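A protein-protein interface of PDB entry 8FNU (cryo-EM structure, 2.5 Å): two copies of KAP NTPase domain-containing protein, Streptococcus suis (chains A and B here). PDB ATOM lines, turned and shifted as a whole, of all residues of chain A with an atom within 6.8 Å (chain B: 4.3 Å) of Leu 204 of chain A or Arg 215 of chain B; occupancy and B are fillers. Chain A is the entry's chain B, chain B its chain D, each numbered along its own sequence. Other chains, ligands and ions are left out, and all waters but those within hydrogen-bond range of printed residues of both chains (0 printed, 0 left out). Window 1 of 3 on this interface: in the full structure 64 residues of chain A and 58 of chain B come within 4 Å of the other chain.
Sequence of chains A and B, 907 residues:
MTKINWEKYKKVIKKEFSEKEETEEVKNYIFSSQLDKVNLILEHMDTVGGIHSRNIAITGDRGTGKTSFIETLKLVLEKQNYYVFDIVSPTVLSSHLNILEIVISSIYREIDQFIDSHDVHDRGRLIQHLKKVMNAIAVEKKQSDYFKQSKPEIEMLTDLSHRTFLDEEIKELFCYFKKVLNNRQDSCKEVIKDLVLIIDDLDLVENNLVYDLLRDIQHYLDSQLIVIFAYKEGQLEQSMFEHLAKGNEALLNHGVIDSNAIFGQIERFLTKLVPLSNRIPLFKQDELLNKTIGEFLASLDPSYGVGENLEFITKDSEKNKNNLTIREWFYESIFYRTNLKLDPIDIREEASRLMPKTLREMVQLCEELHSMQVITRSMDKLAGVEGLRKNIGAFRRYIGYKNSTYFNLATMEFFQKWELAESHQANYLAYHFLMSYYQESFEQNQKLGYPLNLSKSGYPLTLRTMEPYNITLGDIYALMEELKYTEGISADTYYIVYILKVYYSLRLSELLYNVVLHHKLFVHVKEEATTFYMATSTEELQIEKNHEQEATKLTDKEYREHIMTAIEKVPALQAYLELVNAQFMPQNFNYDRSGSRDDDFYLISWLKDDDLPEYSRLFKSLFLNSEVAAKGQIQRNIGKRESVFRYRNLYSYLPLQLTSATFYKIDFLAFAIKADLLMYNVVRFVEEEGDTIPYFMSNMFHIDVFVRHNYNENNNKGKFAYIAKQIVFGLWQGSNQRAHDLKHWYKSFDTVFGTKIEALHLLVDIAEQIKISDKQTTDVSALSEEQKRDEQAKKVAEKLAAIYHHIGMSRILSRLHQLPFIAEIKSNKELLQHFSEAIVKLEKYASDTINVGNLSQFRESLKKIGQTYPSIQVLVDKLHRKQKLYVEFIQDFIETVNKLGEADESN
The guanidinium group (NE) of Arg 215 of chain B lies within hydrogen-bond range of the side-chain hydroxyl (OH) of Tyr 211 of chain B (3.0 Å).
OG of Ser 94 of chain A lies within hydrogen-bond range of O of Pro 90 of chain A (3.3 Å).
The side-chain amide oxygen (OE1) of Gln 218 of chain B lies within hydrogen-bond range of the guanidinium group (NH1) of Arg 215 of chain B.
Among the printed residues, merely in contact across the chains: Pro 90 of chain A with Gln 218 of chain B, Pro 90 of chain A with His 219 of chain B, Ser 94 of chain A with His 219 of chain B, Leu 204 of chain A with Arg 215 of chain B, Leu 204 of chain A with Gln 265 of chain B, Leu 204 of chain A with Phe 269 of chain B and Glu 206 of chain A with Arg 215 of chain B.
Of chain A, only Leu 204 and Glu 206 come within 4 Å of Arg 215 of chain B.
Printed residues of chain B within 4 Å of Pro 90 of chain A: Gln 218 and His 219.
Of the printed residues of chain A, Phe 269 of chain B touches Leu 204.
Of the printed residues of chain A, Gln 218 of chain B touches Pro 90.
Printed residues of chain B within 4 Å of Ser 94 of chain A: His 219.
Of the printed residues of chain A, His 219 of chain B touches Pro 90 and Ser 94.
Ile 217 of chain B touches none of the printed residues of chain A.
The nearest residue of chain A that does not touch Arg 215 of chain B is Val 205 of chain A (5.0 Å).
Of the 12 printed residues of chain A, 4 touch a printed residue of chain B.
Hydrophobic or aromatic side chains of chain A that line the printed part of chain B: Pro 90 and Leu 204.
Hydrophobic or aromatic side chains of chain B within 4 Å of the printed part of chain A: His 219 and Phe 269.
No position is printed for both chains.
Of the 7 pairs that touch across the chains among the printed residues, none has its exchanged pair printed and touching as well.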
ATOM      1  N   PRO A  90     -18.104  15.001   9.329  1.00  0.00           N
ATOM      2  CA  PRO A  90     -16.777  14.414   9.562  1.00  0.00           C
ATOM      3  C   PRO A  90     -16.235  13.690   8.346  1.00  0.00           C
ATOM      4  O   PRO A  90     -15.013  13.599   8.182  1.00  0.00           O
ATOM      5  CB  PRO A  90     -17.025  13.460  10.737  1.00  0.00           C
ATOM      6  CG  PRO A  90     -18.160  14.075  11.469  1.00  0.00           C
ATOM      7  CD  PRO A  90     -19.048  14.665  10.409  1.00  0.00           C
ATOM      8  N   SER A  94     -12.595  14.599   6.970  1.00  0.00           N
ATOM      9  CA  SER A  94     -11.602  13.540   6.855  1.00  0.00           C
ATOM     10  C   SER A  94     -10.882  13.563   5.514  1.00  0.00           C
ATOM     11  O   SER A  94      -9.900  12.833   5.345  1.00  0.00           O
ATOM     12  CB  SER A  94     -12.264  12.178   7.062  1.00  0.00           C
ATOM     13  OG  SER A  94     -13.197  11.898   6.034  1.00  0.00           O
ATOM     14  N   ASP A 201     -21.694  17.396  13.489  1.00  0.00           N
ATOM     15  CA  ASP A 201     -21.053  16.229  14.093  1.00  0.00           C
ATOM     16  C   ASP A 201     -19.587  16.512  14.411  1.00  0.00           C
ATOM     17  O   ASP A 201     -18.719  15.650  14.257  1.00  0.00           O
ATOM     18  CB  ASP A 201     -21.193  15.003  13.189  1.00  0.00           C
ATOM     19  CG  ASP A 201     -22.578  14.391  13.246  1.00  0.00           C
ATOM     20  OD1 ASP A 201     -22.739  13.239  12.793  1.00  0.00           O
ATOM     21  OD2 ASP A 201     -23.504  15.059  13.751  1.00  0.00           O
ATOM     22  N   LEU A 202     -19.311  17.733  14.857  1.00  0.00           N
ATOM     23  CA  LEU A 202     -17.981  18.110  15.314  1.00  0.00           C
ATOM     24  C   LEU A 202     -17.685  17.611  16.721  1.00  0.00           C
ATOM     25  O   LEU A 202     -16.574  17.826  17.216  1.00  0.00           O
ATOM     26  CB  LEU A 202     -17.824  19.632  15.269  1.00  0.00           C
ATOM     27  CG  LEU A 202     -16.412  20.178  15.050  1.00  0.00           C
ATOM     28  CD1 LEU A 202     -15.884  19.802  13.675  1.00  0.00           C
ATOM     29  CD2 LEU A 202     -16.403  21.684  15.236  1.00  0.00           C
ATOM     30  N   ASP A 203     -18.650  16.952  17.370  1.00  0.00           N
ATOM     31  CA  ASP A 203     -18.452  16.502  18.743  1.00  0.00           C
ATOM     32  C   ASP A 203     -17.212  15.633  18.874  1.00  0.00           C
ATOM     33  O   ASP A 203     -16.558  15.638  19.923  1.00  0.00           O
ATOM     34  CB  ASP A 203     -19.680  15.729  19.223  1.00  0.00           C
ATOM     35  CG  ASP A 203     -20.972  16.477  18.974  1.00  0.00           C
ATOM     36  OD1 ASP A 203     -20.926  17.716  18.831  1.00  0.00           O
ATOM     37  OD2 ASP A 203     -22.037  15.824  18.922  1.00  0.00           O
ATOM     38  N   LEU A 204     -16.873  14.878  17.829  1.00  0.00           N
ATOM     39  CA  LEU A 204     -15.704  13.999  17.869  1.00  0.00           C
ATOM     40  C   LEU A 204     -15.120  13.936  16.456  1.00  0.00           C
ATOM     41  O   LEU A 204     -15.525  13.105  15.641  1.00  0.00           O
ATOM     42  CB  LEU A 204     -16.090  12.621  18.384  1.00  0.00           C
ATOM     43  CG  LEU A 204     -14.947  11.669  18.732  1.00  0.00           C
ATOM     44  CD1 LEU A 204     -15.332  10.767  19.880  1.00  0.00           C
ATOM     45  CD2 LEU A 204     -14.581  10.840  17.531  1.00  0.00           C
ATOM     46  N   VAL A 205     -14.169  14.828  16.178  1.00  0.00           N
ATOM     47  CA  VAL A 205     -13.434  14.833  14.911  1.00  0.00           C
ATOM     48  C   VAL A 205     -11.950  14.924  15.253  1.00  0.00           C
ATOM     49  O   VAL A 205     -11.378  16.017  15.322  1.00  0.00           O
ATOM     50  CB  VAL A 205     -13.861  15.979  13.988  1.00  0.00           C
ATOM     51  CG1 VAL A 205     -13.068  15.946  12.695  1.00  0.00           C
ATOM     52  CG2 VAL A 205     -15.350  15.899  13.700  1.00  0.00           C
ATOM     53  N   GLU A 206     -11.315  13.771  15.463  1.00  0.00           N
ATOM     54  CA  GLU A 206      -9.860  13.640  15.520  1.00  0.00           C
ATOM     55  C   GLU A 206      -9.177  14.769  16.286  1.00  0.00           C
ATOM     56  O   GLU A 206      -8.037  15.128  15.975  1.00  0.00           O
ATOM     57  CB  GLU A 206      -9.293  13.561  14.100  1.00  0.00           C
ATOM     58  CG  GLU A 206      -8.023  12.721  13.979  1.00  0.00           C
ATOM     59  CD  GLU A 206      -6.756  13.558  13.946  1.00  0.00           C
ATOM     60  OE1 GLU A 206      -6.798  14.695  13.431  1.00  0.00           O
ATOM     61  OE2 GLU A 206      -5.714  13.074  14.436  1.00  0.00           O
ATOM     62  N   ASN A 207      -9.853  15.327  17.290  1.00  0.00           N
ATOM     63  CA  ASN A 207      -9.263  16.350  18.148  1.00  0.00           C
ATOM     64  C   ASN A 207      -8.597  17.464  17.341  1.00  0.00           C
ATOM     65  O   ASN A 207      -9.285  18.366  16.849  1.00  0.00           O
ATOM     66  CB  ASN A 207      -8.269  15.711  19.121  1.00  0.00           C
ATOM     67  CG  ASN A 207      -7.843  16.662  20.223  1.00  0.00           C
ATOM     68  OD1 ASN A 207      -6.675  17.037  20.319  1.00  0.00           O
ATOM     69  ND2 ASN A 207      -8.794  17.060  21.061  1.00  0.00           N
ATOM     70  N   VAL A 210     -10.076  19.695  14.374  1.00  0.00           N
ATOM     71  CA  VAL A 210     -10.983  20.826  14.548  1.00  0.00           C
ATOM     72  C   VAL A 210     -10.193  22.100  14.811  1.00  0.00           C
ATOM     73  O   VAL A 210     -10.593  23.187  14.376  1.00  0.00           O
ATOM     74  CB  VAL A 210     -12.009  20.545  15.667  1.00  0.00           C
ATOM     75  CG1 VAL A 210     -12.656  19.179  15.479  1.00  0.00           C
ATOM     76  CG2 VAL A 210     -11.373  20.655  17.039  1.00  0.00           C
ATOM     77  N   LYS A 232     -19.737  20.367  21.002  1.00  0.00           N
ATOM     78  CA  LYS A 232     -20.272  20.047  22.318  1.00  0.00           C
ATOM     79  C   LYS A 232     -19.392  20.624  23.421  1.00  0.00           C
ATOM     80  O   LYS A 232     -18.161  20.598  23.328  1.00  0.00           O
ATOM     81  CB  LYS A 232     -20.413  18.530  22.509  1.00  0.00           C
ATOM     82  CG  LYS A 232     -19.098  17.753  22.527  1.00  0.00           C
ATOM     83  CD  LYS A 232     -19.134  16.603  23.527  1.00  0.00           C
ATOM     84  CE  LYS A 232     -19.283  17.114  24.953  1.00  0.00           C
ATOM     85  NZ  LYS A 232     -18.884  16.122  25.982  1.00  0.00           N
ATOM     86  N   GLN A 235     -15.207  21.381  23.825  1.00  0.00           N
ATOM     87  CA  GLN A 235     -14.307  20.712  22.890  1.00  0.00           C
ATOM     88  C   GLN A 235     -13.341  21.701  22.252  1.00  0.00           C
ATOM     89  O   GLN A 235     -12.155  21.396  22.073  1.00  0.00           O
ATOM     90  CB  GLN A 235     -15.129  19.991  21.822  1.00  0.00           C
ATOM     91  CG  GLN A 235     -14.315  19.238  20.791  1.00  0.00           C
ATOM     92  CD  GLN A 235     -15.191  18.549  19.767  1.00  0.00           C
ATOM     93  OE1 GLN A 235     -16.416  18.656  19.813  1.00  0.00           O
ATOM     94  NE2 GLN A 235     -14.568  17.838  18.837  1.00  0.00           N
ATOM     95  N   TYR B 211      -8.596   0.875  14.701  1.00  0.00           N
ATOM     96  CA  TYR B 211      -8.995   2.275  14.784  1.00  0.00           C
ATOM     97  C   TYR B 211      -9.100   2.880  13.391  1.00  0.00           C
ATOM     98  O   TYR B 211     -10.126   3.470  13.033  1.00  0.00           O
ATOM     99  CB  TYR B 211      -8.002   3.061  15.644  1.00  0.00           C
ATOM    100  CG  TYR B 211      -8.268   4.549  15.680  1.00  0.00           C
ATOM    101  CD1 TYR B 211      -9.192   5.088  16.562  1.00  0.00           C
ATOM    102  CD2 TYR B 211      -7.597   5.413  14.826  1.00  0.00           C
ATOM    103  CE1 TYR B 211      -9.436   6.446  16.595  1.00  0.00           C
ATOM    104  CE2 TYR B 211      -7.836   6.770  14.851  1.00  0.00           C
ATOM    105  CZ  TYR B 211      -8.756   7.282  15.738  1.00  0.00           C
ATOM    106  OH  TYR B 211      -8.998   8.635  15.767  1.00  0.00           O
ATOM    107  N   ASP B 212      -8.056   2.706  12.576  1.00  0.00           N
ATOM    108  CA  ASP B 212      -8.121   3.178  11.198  1.00  0.00           C
ATOM    109  C   ASP B 212      -9.309   2.571  10.470  1.00  0.00           C
ATOM    110  O   ASP B 212      -9.926   3.230   9.627  1.00  0.00           O
ATOM    111  CB  ASP B 212      -6.821   2.844  10.464  1.00  0.00           C
ATOM    112  CG  ASP B 212      -5.671   3.744  10.873  1.00  0.00           C
ATOM    113  OD1 ASP B 212      -5.920   4.758  11.559  1.00  0.00           O
ATOM    114  OD2 ASP B 212      -4.518   3.436  10.508  1.00  0.00           O
ATOM    115  N   LEU B 213      -9.646   1.319  10.784  1.00  0.00           N
ATOM    116  CA  LEU B 213     -10.844   0.713  10.220  1.00  0.00           C
ATOM    117  C   LEU B 213     -12.092   1.456  10.679  1.00  0.00           C
ATOM    118  O   LEU B 213     -12.931   1.852   9.860  1.00  0.00           O
ATOM    119  CB  LEU B 213     -10.911  -0.763  10.617  1.00  0.00           C
ATOM    120  CG  LEU B 213     -12.084  -1.591  10.096  1.00  0.00           C
ATOM    121  CD1 LEU B 213     -12.026  -1.716   8.587  1.00  0.00           C
ATOM    122  CD2 LEU B 213     -12.083  -2.961  10.751  1.00  0.00           C
ATOM    123  N   LEU B 214     -12.212   1.690  11.989  1.00  0.00           N
ATOM    124  CA  LEU B 214     -13.424   2.301  12.524  1.00  0.00           C
ATOM    125  C   LEU B 214     -13.705   3.633  11.845  1.00  0.00           C
ATOM    126  O   LEU B 214     -14.804   3.863  11.327  1.00  0.00           O
ATOM    127  CB  LEU B 214     -13.293   2.486  14.035  1.00  0.00           C
ATOM    128  CG  LEU B 214     -13.319   1.208  14.874  1.00  0.00           C
ATOM    129  CD1 LEU B 214     -13.037   1.523  16.334  1.00  0.00           C
ATOM    130  CD2 LEU B 214     -14.652   0.495  14.727  1.00  0.00           C
ATOM    131  N   ARG B 215     -12.708   4.518  11.819  1.00  0.00           N
ATOM    132  CA  ARG B 215     -12.872   5.791  11.130  1.00  0.00           C
ATOM    133  C   ARG B 215     -13.313   5.575   9.692  1.00  0.00           C
ATOM    134  O   ARG B 215     -14.251   6.225   9.216  1.00  0.00           O
ATOM    135  CB  ARG B 215     -11.564   6.578  11.175  1.00  0.00           C
ATOM    136  CG  ARG B 215     -11.143   6.999  12.564  1.00  0.00           C
ATOM    137  CD  ARG B 215     -12.199   7.853  13.225  1.00  0.00           C
ATOM    138  NE  ARG B 215     -11.696   8.488  14.435  1.00  0.00           N
ATOM    139  CZ  ARG B 215     -12.362   9.398  15.129  1.00  0.00           C
ATOM    140  NH1 ARG B 215     -13.576   9.788  14.774  1.00  0.00           N
ATOM    141  NH2 ARG B 215     -11.794   9.932  16.205  1.00  0.00           N
ATOM    142  N   ASP B 216     -12.664   4.644   8.990  1.00  0.00           N
ATOM    143  CA  ASP B 216     -13.038   4.385   7.607  1.00  0.00           C
ATOM    144  C   ASP B 216     -14.499   3.972   7.514  1.00  0.00           C
ATOM    145  O   ASP B 216     -15.205   4.353   6.574  1.00  0.00           O
ATOM    146  CB  ASP B 216     -12.129   3.309   7.015  1.00  0.00           C
ATOM    147  CG  ASP B 216     -10.728   3.820   6.736  1.00  0.00           C
ATOM    148  OD1 ASP B 216     -10.557   5.051   6.612  1.00  0.00           O
ATOM    149  OD2 ASP B 216      -9.800   2.992   6.638  1.00  0.00           O
ATOM    150  N   ILE B 217     -14.977   3.193   8.482  1.00  0.00           N
ATOM    151  CA  ILE B 217     -16.388   2.833   8.484  1.00  0.00           C
ATOM    152  C   ILE B 217     -17.243   4.040   8.840  1.00  0.00           C
ATOM    153  O   ILE B 217     -18.324   4.242   8.275  1.00  0.00           O
ATOM    154  CB  ILE B 217     -16.623   1.653   9.438  1.00  0.00           C
ATOM    155  CG1 ILE B 217     -15.904   0.420   8.888  1.00  0.00           C
ATOM    156  CG2 ILE B 217     -18.113   1.397   9.601  1.00  0.00           C
ATOM    157  CD1 ILE B 217     -15.784  -0.708   9.868  1.00  0.00           C
ATOM    158  N   GLN B 218     -16.776   4.866   9.776  1.00  0.00           N
ATOM    159  CA  GLN B 218     -17.517   6.074  10.112  1.00  0.00           C
ATOM    160  C   GLN B 218     -17.620   6.993   8.909  1.00  0.00           C
ATOM    161  O   GLN B 218     -18.685   7.561   8.638  1.00  0.00           O
ATOM    162  CB  GLN B 218     -16.838   6.804  11.271  1.00  0.00           C
ATOM    163  CG  GLN B 218     -17.462   8.153  11.636  1.00  0.00           C
ATOM    164  CD  GLN B 218     -16.507   9.048  12.403  1.00  0.00           C
ATOM    165  OE1 GLN B 218     -15.327   8.733  12.555  1.00  0.00           O
ATOM    166  NE2 GLN B 218     -17.014  10.173  12.893  1.00  0.00           N
ATOM    167  N   HIS B 219     -16.518   7.162   8.185  1.00  0.00           N
ATOM    168  CA  HIS B 219     -16.500   8.132   7.106  1.00  0.00           C
ATOM    169  C   HIS B 219     -17.127   7.596   5.830  1.00  0.00           C
ATOM    170  O   HIS B 219     -17.835   8.342   5.145  1.00  0.00           O
ATOM    171  CB  HIS B 219     -15.065   8.607   6.844  1.00  0.00           C
ATOM    172  CG  HIS B 219     -14.417   9.240   8.037  1.00  0.00           C
ATOM    173  ND1 HIS B 219     -15.114  10.039   8.917  1.00  0.00           N
ATOM    174  CD2 HIS B 219     -13.144   9.197   8.497  1.00  0.00           C
ATOM    175  CE1 HIS B 219     -14.301  10.457   9.869  1.00  0.00           C
ATOM    176  NE2 HIS B 219     -13.100   9.961   9.637  1.00  0.00           N
ATOM    177  N   MET B 240      -9.580   2.954  20.403  1.00  0.00           N
ATOM    178  CA  MET B 240      -9.850   4.386  20.311  1.00  0.00           C
ATOM    179  C   MET B 240      -9.060   5.168  21.354  1.00  0.00           C
ATOM    180  O   MET B 240      -8.549   6.257  21.066  1.00  0.00           O
ATOM    181  CB  MET B 240     -11.346   4.650  20.474  1.00  0.00           C
ATOM    182  CG  MET B 240     -12.226   3.963  19.444  1.00  0.00           C
ATOM    183  SD  MET B 240     -13.535   5.036  18.824  1.00  0.00           S
ATOM    184  CE  MET B 240     -12.600   6.201  17.835  1.00  0.00           C
ATOM    185  N   GLN B 265     -16.223  10.243  25.246  1.00  0.00           N
ATOM    186  CA  GLN B 265     -16.152  10.478  23.808  1.00  0.00           C
ATOM    187  C   GLN B 265     -16.261   9.166  23.038  1.00  0.00           C
ATOM    188  O   GLN B 265     -17.110   9.012  22.145  1.00  0.00           O
ATOM    189  CB  GLN B 265     -14.835  11.182  23.475  1.00  0.00           C
ATOM    190  CG  GLN B 265     -14.767  12.646  23.871  1.00  0.00           C
ATOM    191  CD  GLN B 265     -13.346  13.178  23.868  1.00  0.00           C
ATOM    192  OE1 GLN B 265     -12.631  13.061  22.872  1.00  0.00           O
ATOM    193  NE2 GLN B 265     -12.927  13.763  24.985  1.00  0.00           N
ATOM    194  N   PHE B 269     -19.393   7.818  20.575  1.00  0.00           N
ATOM    195  CA  PHE B 269     -19.032   7.465  19.203  1.00  0.00           C
ATOM    196  C   PHE B 269     -19.442   6.035  18.884  1.00  0.00           C
ATOM    197  O   PHE B 269     -20.042   5.767  17.839  1.00  0.00           O
ATOM    198  CB  PHE B 269     -17.524   7.632  18.981  1.00  0.00           C
ATOM    199  CG  PHE B 269     -17.034   7.059  17.669  1.00  0.00           C
ATOM    200  CD1 PHE B 269     -17.077   7.812  16.508  1.00  0.00           C
ATOM    201  CD2 PHE B 269     -16.540   5.763  17.596  1.00  0.00           C
ATOM    202  CE1 PHE B 269     -16.633   7.289  15.306  1.00  0.00           C
ATOM    203  CE2 PHE B 269     -16.097   5.239  16.394  1.00  0.00           C
ATOM    204  CZ  PHE B 269     -16.144   6.002  15.251  1.00  0.00           C
